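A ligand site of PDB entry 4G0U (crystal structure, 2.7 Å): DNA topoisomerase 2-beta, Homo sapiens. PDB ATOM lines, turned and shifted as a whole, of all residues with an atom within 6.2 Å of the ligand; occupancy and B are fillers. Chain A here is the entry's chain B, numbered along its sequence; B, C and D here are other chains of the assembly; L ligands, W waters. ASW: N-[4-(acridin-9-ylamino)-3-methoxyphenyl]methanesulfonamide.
N14 of the ligand lies close to O of Arg 85 (3.3 Å). OE2 of Glu 104 is in hydrogen-bond range of N6 of the ligand (2.8 Å). The backbone NH of Gly 86 lies within hydrogen-bond range of an oxygen (O2) of the ligand (3.3 Å).
The guanidinium group (NH1) of Arg 85 sits at hydrogen-bond distance from the backbone carbonyl oxygen (O) of Gly 35 (3.1 Å). N2 of DG 5 of chain C lies close to O2 of DC 8 of chain D, at 2.6 Å. ND2 of Asn 107 is in hydrogen-bond range of O of Ala 103. O2 of DC 8 of chain D is in hydrogen-bond range of the backbone NH of Lys 87 (3.0 Å).
A nitrogen (N22) of the ligand lies close to O6 of DG 5 of chain C. Ile 36 touches the ligand (CG2 to C8, 3.7 Å). Pro 37 touches the ligand (CD to C8, 3.5 Å). Lys 87 touches the ligand (O to C1, 3.3 Å). Ala 103 touches the ligand (CB to C8, 3.5 Å). NE2 of Gln 360 touches C19 of the ligand, at 3.4 Å. N1 of DT 1 of chain B touches C18 of the ligand, at 3.2 Å. DA 4 of chain C touches the ligand. C5 of DC 8 of chain D touches C19 of the ligand (3.5 Å). Hydrophobic or aromatic side chains that line the ligand: Ile 36, Pro 37 and Ala 103. Within 4 Å of the ligand: Ile 36, Pro 37, Arg 85, Gly 86, Lys 87, Ala 103, Glu 104, Gln 360, DT 1 of chain B, DA 4 of chain C, DG 5 of chain C and DC 8 of chain D. The nearest printed residue that does not touch the ligand is Ile 88 (4.2 Å).
Water W1 lies within hydrogen-bond range of N3 of DG 5 of chain C (3.0 Å) and O2 of the ligand (3.4 Å).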
ATOM      1  N   GLY A  35     -33.048  -6.332  -6.762  1.00  0.00           N
ATOM      2  CA  GLY A  35     -32.535  -5.429  -5.742  1.00  0.00           C
ATOM      3  C   GLY A  35     -31.614  -4.339  -6.276  1.00  0.00           C
ATOM      4  O   GLY A  35     -30.553  -4.057  -5.719  1.00  0.00           O
ATOM      5  N   ILE A  36     -32.026  -3.699  -7.373  1.00  0.00           N
ATOM      6  CA  ILE A  36     -31.247  -2.626  -7.981  1.00  0.00           C
ATOM      7  C   ILE A  36     -31.326  -1.359  -7.113  1.00  0.00           C
ATOM      8  O   ILE A  36     -32.148  -1.291  -6.203  1.00  0.00           O
ATOM      9  CB  ILE A  36     -31.740  -2.325  -9.418  1.00  0.00           C
ATOM     10  CG1 ILE A  36     -33.256  -2.163  -9.449  1.00  0.00           C
ATOM     11  CG2 ILE A  36     -31.314  -3.421 -10.362  1.00  0.00           C
ATOM     12  CD1 ILE A  36     -33.765  -1.641 -10.776  1.00  0.00           C
ATOM     13  N   PRO A  37     -30.417  -0.379  -7.369  1.00  0.00           N
ATOM     14  CA  PRO A  37     -30.493   0.923  -6.691  1.00  0.00           C
ATOM     15  C   PRO A  37     -31.868   1.589  -6.861  1.00  0.00           C
ATOM     16  O   PRO A  37     -32.456   1.545  -7.958  1.00  0.00           O
ATOM     17  CB  PRO A  37     -29.407   1.727  -7.383  1.00  0.00           C
ATOM     18  CG  PRO A  37     -28.376   0.711  -7.708  1.00  0.00           C
ATOM     19  CD  PRO A  37     -29.129  -0.537  -8.069  1.00  0.00           C
ATOM     20  N   LEU A  84     -24.931   5.544  -5.832  1.00  0.00           N
ATOM     21  CA  LEU A  84     -24.038   4.930  -6.794  1.00  0.00           C
ATOM     22  C   LEU A  84     -23.280   3.868  -6.035  1.00  0.00           C
ATOM     23  O   LEU A  84     -22.763   4.126  -4.965  1.00  0.00           O
ATOM     24  CB  LEU A  84     -23.082   5.969  -7.367  1.00  0.00           C
ATOM     25  CG  LEU A  84     -23.825   7.111  -8.033  1.00  0.00           C
ATOM     26  CD1 LEU A  84     -22.865   8.182  -8.518  1.00  0.00           C
ATOM     27  CD2 LEU A  84     -24.665   6.573  -9.182  1.00  0.00           C
ATOM     28  N   ARG A  85     -23.220   2.661  -6.575  1.00  0.00           N
ATOM     29  CA  ARG A  85     -22.662   1.540  -5.836  1.00  0.00           C
ATOM     30  C   ARG A  85     -21.203   1.258  -6.107  1.00  0.00           C
ATOM     31  O   ARG A  85     -20.669   0.279  -5.593  1.00  0.00           O
ATOM     32  CB  ARG A  85     -23.512   0.290  -6.029  1.00  0.00           C
ATOM     33  CG  ARG A  85     -24.617   0.227  -5.004  1.00  0.00           C
ATOM     34  CD  ARG A  85     -25.615  -0.841  -5.287  1.00  0.00           C
ATOM     35  NE  ARG A  85     -26.793  -0.637  -4.472  1.00  0.00           N
ATOM     36  CZ  ARG A  85     -27.873  -1.403  -4.540  1.00  0.00           C
ATOM     37  NH1 ARG A  85     -27.900  -2.417  -5.391  1.00  0.00           N
ATOM     38  NH2 ARG A  85     -28.915  -1.161  -3.758  1.00  0.00           N
ATOM     39  N   GLY A  86     -20.559   2.120  -6.888  1.00  0.00           N
ATOM     40  CA  GLY A  86     -19.135   1.988  -7.138  1.00  0.00           C
ATOM     41  C   GLY A  86     -18.721   2.817  -8.320  1.00  0.00           C
ATOM     42  O   GLY A  86     -19.464   3.718  -8.738  1.00  0.00           O
ATOM     43  N   LYS A  87     -17.535   2.537  -8.869  1.00  0.00           N
ATOM     44  CA  LYS A  87     -17.028   3.272 -10.026  1.00  0.00           C
ATOM     45  C   LYS A  87     -17.991   3.109 -11.192  1.00  0.00           C
ATOM     46  O   LYS A  87     -18.604   2.064 -11.359  1.00  0.00           O
ATOM     47  CB  LYS A  87     -15.612   2.810 -10.414  1.00  0.00           C
ATOM     48  CG  LYS A  87     -14.579   2.939  -9.327  1.00  0.00           C
ATOM     49  CD  LYS A  87     -14.611   4.318  -8.713  1.00  0.00           C
ATOM     50  CE  LYS A  87     -13.694   4.431  -7.517  1.00  0.00           C
ATOM     51  NZ  LYS A  87     -12.264   4.198  -7.875  1.00  0.00           N
ATOM     52  N   ILE A  88     -18.138   4.163 -11.982  1.00  0.00           N
ATOM     53  CA  ILE A  88     -19.099   4.154 -13.056  1.00  0.00           C
ATOM     54  C   ILE A  88     -18.387   4.308 -14.395  1.00  0.00           C
ATOM     55  O   ILE A  88     -17.182   4.525 -14.435  1.00  0.00           O
ATOM     56  CB  ILE A  88     -20.151   5.261 -12.911  1.00  0.00           C
ATOM     57  CG1 ILE A  88     -19.513   6.632 -13.150  1.00  0.00           C
ATOM     58  CG2 ILE A  88     -20.866   5.170 -11.563  1.00  0.00           C
ATOM     59  CD1 ILE A  88     -20.462   7.774 -13.061  1.00  0.00           C
ATOM     60  N   ALA A 103     -26.384   0.871 -16.533  1.00  0.00           N
ATOM     61  CA  ALA A 103     -27.409   1.136 -15.524  1.00  0.00           C
ATOM     62  C   ALA A 103     -27.347   2.533 -14.907  1.00  0.00           C
ATOM     63  O   ALA A 103     -28.363   3.232 -14.871  1.00  0.00           O
ATOM     64  CB  ALA A 103     -27.354   0.102 -14.424  1.00  0.00           C
ATOM     65  N   GLU A 104     -26.173   2.924 -14.411  1.00  0.00           N
ATOM     66  CA  GLU A 104     -26.042   4.158 -13.649  1.00  0.00           C
ATOM     67  C   GLU A 104     -26.279   5.366 -14.526  1.00  0.00           C
ATOM     68  O   GLU A 104     -27.124   6.210 -14.211  1.00  0.00           O
ATOM     69  CB  GLU A 104     -24.664   4.267 -12.993  1.00  0.00           C
ATOM     70  CG  GLU A 104     -24.536   3.532 -11.681  1.00  0.00           C
ATOM     71  CD  GLU A 104     -24.751   2.037 -11.835  1.00  0.00           C
ATOM     72  OE1 GLU A 104     -24.194   1.453 -12.811  1.00  0.00           O
ATOM     73  OE2 GLU A 104     -25.489   1.458 -10.992  1.00  0.00           O
ATOM     74  N   ASN A 107     -29.971   5.577 -15.496  1.00  0.00           N
ATOM     75  CA  ASN A 107     -30.847   6.009 -14.414  1.00  0.00           C
ATOM     76  C   ASN A 107     -30.705   7.504 -14.131  1.00  0.00           C
ATOM     77  O   ASN A 107     -31.708   8.180 -13.892  1.00  0.00           O
ATOM     78  CB  ASN A 107     -30.599   5.186 -13.147  1.00  0.00           C
ATOM     79  CG  ASN A 107     -31.213   3.807 -13.220  1.00  0.00           C
ATOM     80  OD1 ASN A 107     -32.259   3.619 -13.828  1.00  0.00           O
ATOM     81  ND2 ASN A 107     -30.548   2.826 -12.622  1.00  0.00           N
ATOM     82  N   GLN A 360     -13.349  -7.662   0.746  1.00  0.00           N
ATOM     83  CA  GLN A 360     -13.491  -8.604  -0.370  1.00  0.00           C
ATOM     84  C   GLN A 360     -12.370  -8.417  -1.407  1.00  0.00           C
ATOM     85  O   GLN A 360     -11.989  -9.370  -2.103  1.00  0.00           O
ATOM     86  CB  GLN A 360     -14.880  -8.538  -1.019  1.00  0.00           C
ATOM     87  CG  GLN A 360     -15.100  -7.436  -2.062  1.00  0.00           C
ATOM     88  CD  GLN A 360     -15.100  -6.004  -1.469  1.00  0.00           C
ATOM     89  OE1 GLN A 360     -15.142  -5.818  -0.242  1.00  0.00           O
ATOM     90  NE2 GLN A 360     -15.072  -5.001  -2.350  1.00  0.00           N
ATOM     91  P    DT B   1     -17.505  -1.085   1.466  1.00  0.00           P
ATOM     92  OP1  DT B   1     -16.273  -0.756   0.722  1.00  0.00           O
ATOM     93  OP2  DT B   1     -17.720  -2.480   1.912  1.00  0.00           O
ATOM     94  O5'  DT B   1     -18.779  -0.641   0.604  1.00  0.00           O
ATOM     95  C5'  DT B   1     -18.800   0.570  -0.160  1.00  0.00           C
ATOM     96  C4'  DT B   1     -19.999   0.574  -1.076  1.00  0.00           C
ATOM     97  O4'  DT B   1     -19.771  -0.256  -2.244  1.00  0.00           O
ATOM     98  C3'  DT B   1     -21.250  -0.047  -0.490  1.00  0.00           C
ATOM     99  O3'  DT B   1     -21.914   0.857   0.341  1.00  0.00           O
ATOM    100  C2'  DT B   1     -22.067  -0.337  -1.725  1.00  0.00           C
ATOM    101  C1'  DT B   1     -20.980  -0.917  -2.611  1.00  0.00           C
ATOM    102  N1   DT B   1     -20.750  -2.400  -2.544  1.00  0.00           N
ATOM    103  C2   DT B   1     -21.462  -3.213  -3.425  1.00  0.00           C
ATOM    104  O2   DT B   1     -22.289  -2.778  -4.204  1.00  0.00           O
ATOM    105  N3   DT B   1     -21.179  -4.551  -3.336  1.00  0.00           N
ATOM    106  C4   DT B   1     -20.265  -5.146  -2.486  1.00  0.00           C
ATOM    107  O4   DT B   1     -20.072  -6.358  -2.499  1.00  0.00           O
ATOM    108  C5   DT B   1     -19.557  -4.243  -1.607  1.00  0.00           C
ATOM    109  C7   DT B   1     -18.534  -4.779  -0.646  1.00  0.00           C
ATOM    110  C6   DT B   1     -19.833  -2.935  -1.673  1.00  0.00           C
ATOM    111  P    DA C   4     -23.441 -12.108 -11.791  1.00  0.00           P
ATOM    112  OP1  DA C   4     -23.815 -12.466 -13.185  1.00  0.00           O
ATOM    113  OP2  DA C   4     -22.022 -12.190 -11.351  1.00  0.00           O
ATOM    114  O5'  DA C   4     -24.001 -10.632 -11.482  1.00  0.00           O
ATOM    115  C5'  DA C   4     -25.381 -10.281 -11.666  1.00  0.00           C
ATOM    116  C4'  DA C   4     -25.630  -8.821 -11.284  1.00  0.00           C
ATOM    117  O4'  DA C   4     -25.656  -8.639  -9.845  1.00  0.00           O
ATOM    118  C3'  DA C   4     -24.552  -7.883 -11.791  1.00  0.00           C
ATOM    119  O3'  DA C   4     -25.060  -7.265 -12.940  1.00  0.00           O
ATOM    120  C2'  DA C   4     -24.435  -6.815 -10.723  1.00  0.00           C
ATOM    121  C1'  DA C   4     -24.941  -7.481  -9.460  1.00  0.00           C
ATOM    122  N9   DA C   4     -23.873  -7.872  -8.539  1.00  0.00           N
ATOM    123  C8   DA C   4     -23.118  -9.010  -8.579  1.00  0.00           C
ATOM    124  N7   DA C   4     -22.253  -9.106  -7.601  1.00  0.00           N
ATOM    125  C5   DA C   4     -22.446  -7.946  -6.868  1.00  0.00           C
ATOM    126  C6   DA C   4     -21.833  -7.446  -5.702  1.00  0.00           C
ATOM    127  N6   DA C   4     -20.859  -8.073  -5.049  1.00  0.00           N
ATOM    128  N1   DA C   4     -22.262  -6.263  -5.238  1.00  0.00           N
ATOM    129  C2   DA C   4     -23.243  -5.632  -5.903  1.00  0.00           C
ATOM    130  N3   DA C   4     -23.902  -6.005  -7.005  1.00  0.00           N
ATOM    131  C4   DA C   4     -23.444  -7.181  -7.434  1.00  0.00           C
ATOM    132  P    DG C   5     -24.144  -7.127 -14.239  1.00  0.00           P
ATOM    133  OP1  DG C   5     -25.067  -7.294 -15.394  1.00  0.00           O
ATOM    134  OP2  DG C   5     -22.901  -7.931 -14.087  1.00  0.00           O
ATOM    135  O5'  DG C   5     -23.672  -5.613 -14.196  1.00  0.00           O
ATOM    136  C5'  DG C   5     -22.454  -5.448 -14.831  1.00  0.00           C
ATOM    137  C4'  DG C   5     -22.054  -4.011 -14.850  1.00  0.00           C
ATOM    138  O4'  DG C   5     -21.309  -3.719 -13.624  1.00  0.00           O
ATOM    139  C3'  DG C   5     -21.082  -3.770 -15.973  1.00  0.00           C
ATOM    140  O3'  DG C   5     -21.085  -2.412 -16.236  1.00  0.00           O
ATOM    141  C2'  DG C   5     -19.779  -4.244 -15.341  1.00  0.00           C
ATOM    142  C1'  DG C   5     -19.936  -3.658 -13.940  1.00  0.00           C
ATOM    143  N9   DG C   5     -19.140  -4.328 -12.896  1.00  0.00           N
ATOM    144  C8   DG C   5     -18.785  -5.658 -12.852  1.00  0.00           C
ATOM    145  N7   DG C   5     -18.036  -5.978 -11.814  1.00  0.00           N
ATOM    146  C5   DG C   5     -17.896  -4.755 -11.125  1.00  0.00           C
ATOM    147  C6   DG C   5     -17.207  -4.459  -9.926  1.00  0.00           C
ATOM    148  O6   DG C   5     -16.575  -5.235  -9.195  1.00  0.00           O
ATOM    149  N1   DG C   5     -17.293  -3.113  -9.578  1.00  0.00           N
ATOM    150  C2   DG C   5     -17.970  -2.178 -10.320  1.00  0.00           C
ATOM    151  N2   DG C   5     -17.958  -0.932  -9.843  1.00  0.00           N
ATOM    152  N3   DG C   5     -18.629  -2.438 -11.445  1.00  0.00           N
ATOM    153  C4   DG C   5     -18.550  -3.740 -11.796  1.00  0.00           C
ATOM    154  P    DC D   8     -12.433   0.393  -1.753  1.00  0.00           P
ATOM    155  OP1  DC D   8     -12.206   1.270  -0.576  1.00  0.00           O
ATOM    156  OP2  DC D   8     -12.753  -1.023  -1.559  1.00  0.00           O
ATOM    157  O5'  DC D   8     -13.582   1.034  -2.661  1.00  0.00           O
ATOM    158  C5'  DC D   8     -13.610   2.380  -3.077  1.00  0.00           C
ATOM    159  C4'  DC D   8     -14.771   2.587  -4.040  1.00  0.00           C
ATOM    160  O4'  DC D   8     -14.607   1.703  -5.185  1.00  0.00           O
ATOM    161  C3'  DC D   8     -16.183   2.303  -3.467  1.00  0.00           C
ATOM    162  O3'  DC D   8     -17.148   3.276  -3.879  1.00  0.00           O
ATOM    163  C2'  DC D   8     -16.532   0.950  -4.065  1.00  0.00           C
ATOM    164  C1'  DC D   8     -15.788   0.964  -5.398  1.00  0.00           C
ATOM    165  N1   DC D   8     -15.539  -0.452  -5.827  1.00  0.00           N
ATOM    166  C2   DC D   8     -16.068  -0.923  -7.023  1.00  0.00           C
ATOM    167  O2   DC D   8     -16.703  -0.152  -7.745  1.00  0.00           O
ATOM    168  N3   DC D   8     -15.860  -2.215  -7.376  1.00  0.00           N
ATOM    169  C4   DC D   8     -15.159  -3.016  -6.557  1.00  0.00           C
ATOM    170  N4   DC D   8     -14.987  -4.286  -6.909  1.00  0.00           N
ATOM    171  C5   DC D   8     -14.619  -2.555  -5.328  1.00  0.00           C
ATOM    172  C6   DC D   8     -14.829  -1.278  -4.994  1.00  0.00           C
HETATM  173  C1  ASW L   1     -21.623   1.242 -10.275  1.00  0.00           C
HETATM  174  O2  ASW L   1     -21.357   0.153  -9.468  1.00  0.00           O
HETATM  175  C3  ASW L   1     -22.367  -0.723  -9.164  1.00  0.00           C
HETATM  176  C4  ASW L   1     -23.642  -0.481  -9.653  1.00  0.00           C
HETATM  177  C5  ASW L   1     -24.699  -1.338  -9.377  1.00  0.00           C
HETATM  178  N6  ASW L   1     -25.999  -1.039  -9.913  1.00  0.00           N
HETATM  179  S7  ASW L   1     -26.863  -2.135 -10.753  1.00  0.00           S
HETATM  180  C8  ASW L   1     -28.347  -1.426 -11.388  1.00  0.00           C
HETATM  181  O9  ASW L   1     -27.149  -3.295  -9.949  1.00  0.00           O
HETATM  182  O10 ASW L   1     -26.080  -2.725 -11.805  1.00  0.00           O
HETATM  183  C11 ASW L   1     -24.458  -2.469  -8.599  1.00  0.00           C
HETATM  184  C12 ASW L   1     -23.179  -2.705  -8.094  1.00  0.00           C
HETATM  185  C13 ASW L   1     -22.123  -1.848  -8.370  1.00  0.00           C
HETATM  186  N14 ASW L   1     -20.784  -2.080  -7.880  1.00  0.00           N
HETATM  187  C15 ASW L   1     -20.199  -3.372  -7.608  1.00  0.00           C
HETATM  188  C16 ASW L   1     -19.344  -3.488  -6.456  1.00  0.00           C
HETATM  189  C17 ASW L   1     -19.109  -2.371  -5.630  1.00  0.00           C
HETATM  190  C18 ASW L   1     -18.280  -2.502  -4.517  1.00  0.00           C
HETATM  191  C19 ASW L   1     -17.686  -3.736  -4.212  1.00  0.00           C
HETATM  192  C20 ASW L   1     -17.912  -4.839  -5.039  1.00  0.00           C
HETATM  193  C21 ASW L   1     -18.754  -4.702  -6.176  1.00  0.00           C
HETATM  194  N22 ASW L   1     -18.949  -5.820  -6.968  1.00  0.00           N
HETATM  195  C23 ASW L   1     -19.760  -5.714  -8.088  1.00  0.00           C
HETATM  196  C24 ASW L   1     -19.919  -6.898  -8.856  1.00  0.00           C
HETATM  197  C25 ASW L   1     -20.711  -6.871  -9.989  1.00  0.00           C
HETATM  198  C26 ASW L   1     -21.338  -5.677 -10.360  1.00  0.00           C
HETATM  199  C27 ASW L   1     -21.180  -4.508  -9.611  1.00  0.00           C
HETATM  200  C28 ASW L   1     -20.377  -4.532  -8.451  1.00  0.00           C
HETATM  201  O   HOH W   1     -20.810  -0.827 -12.729  1.00  0.00           O
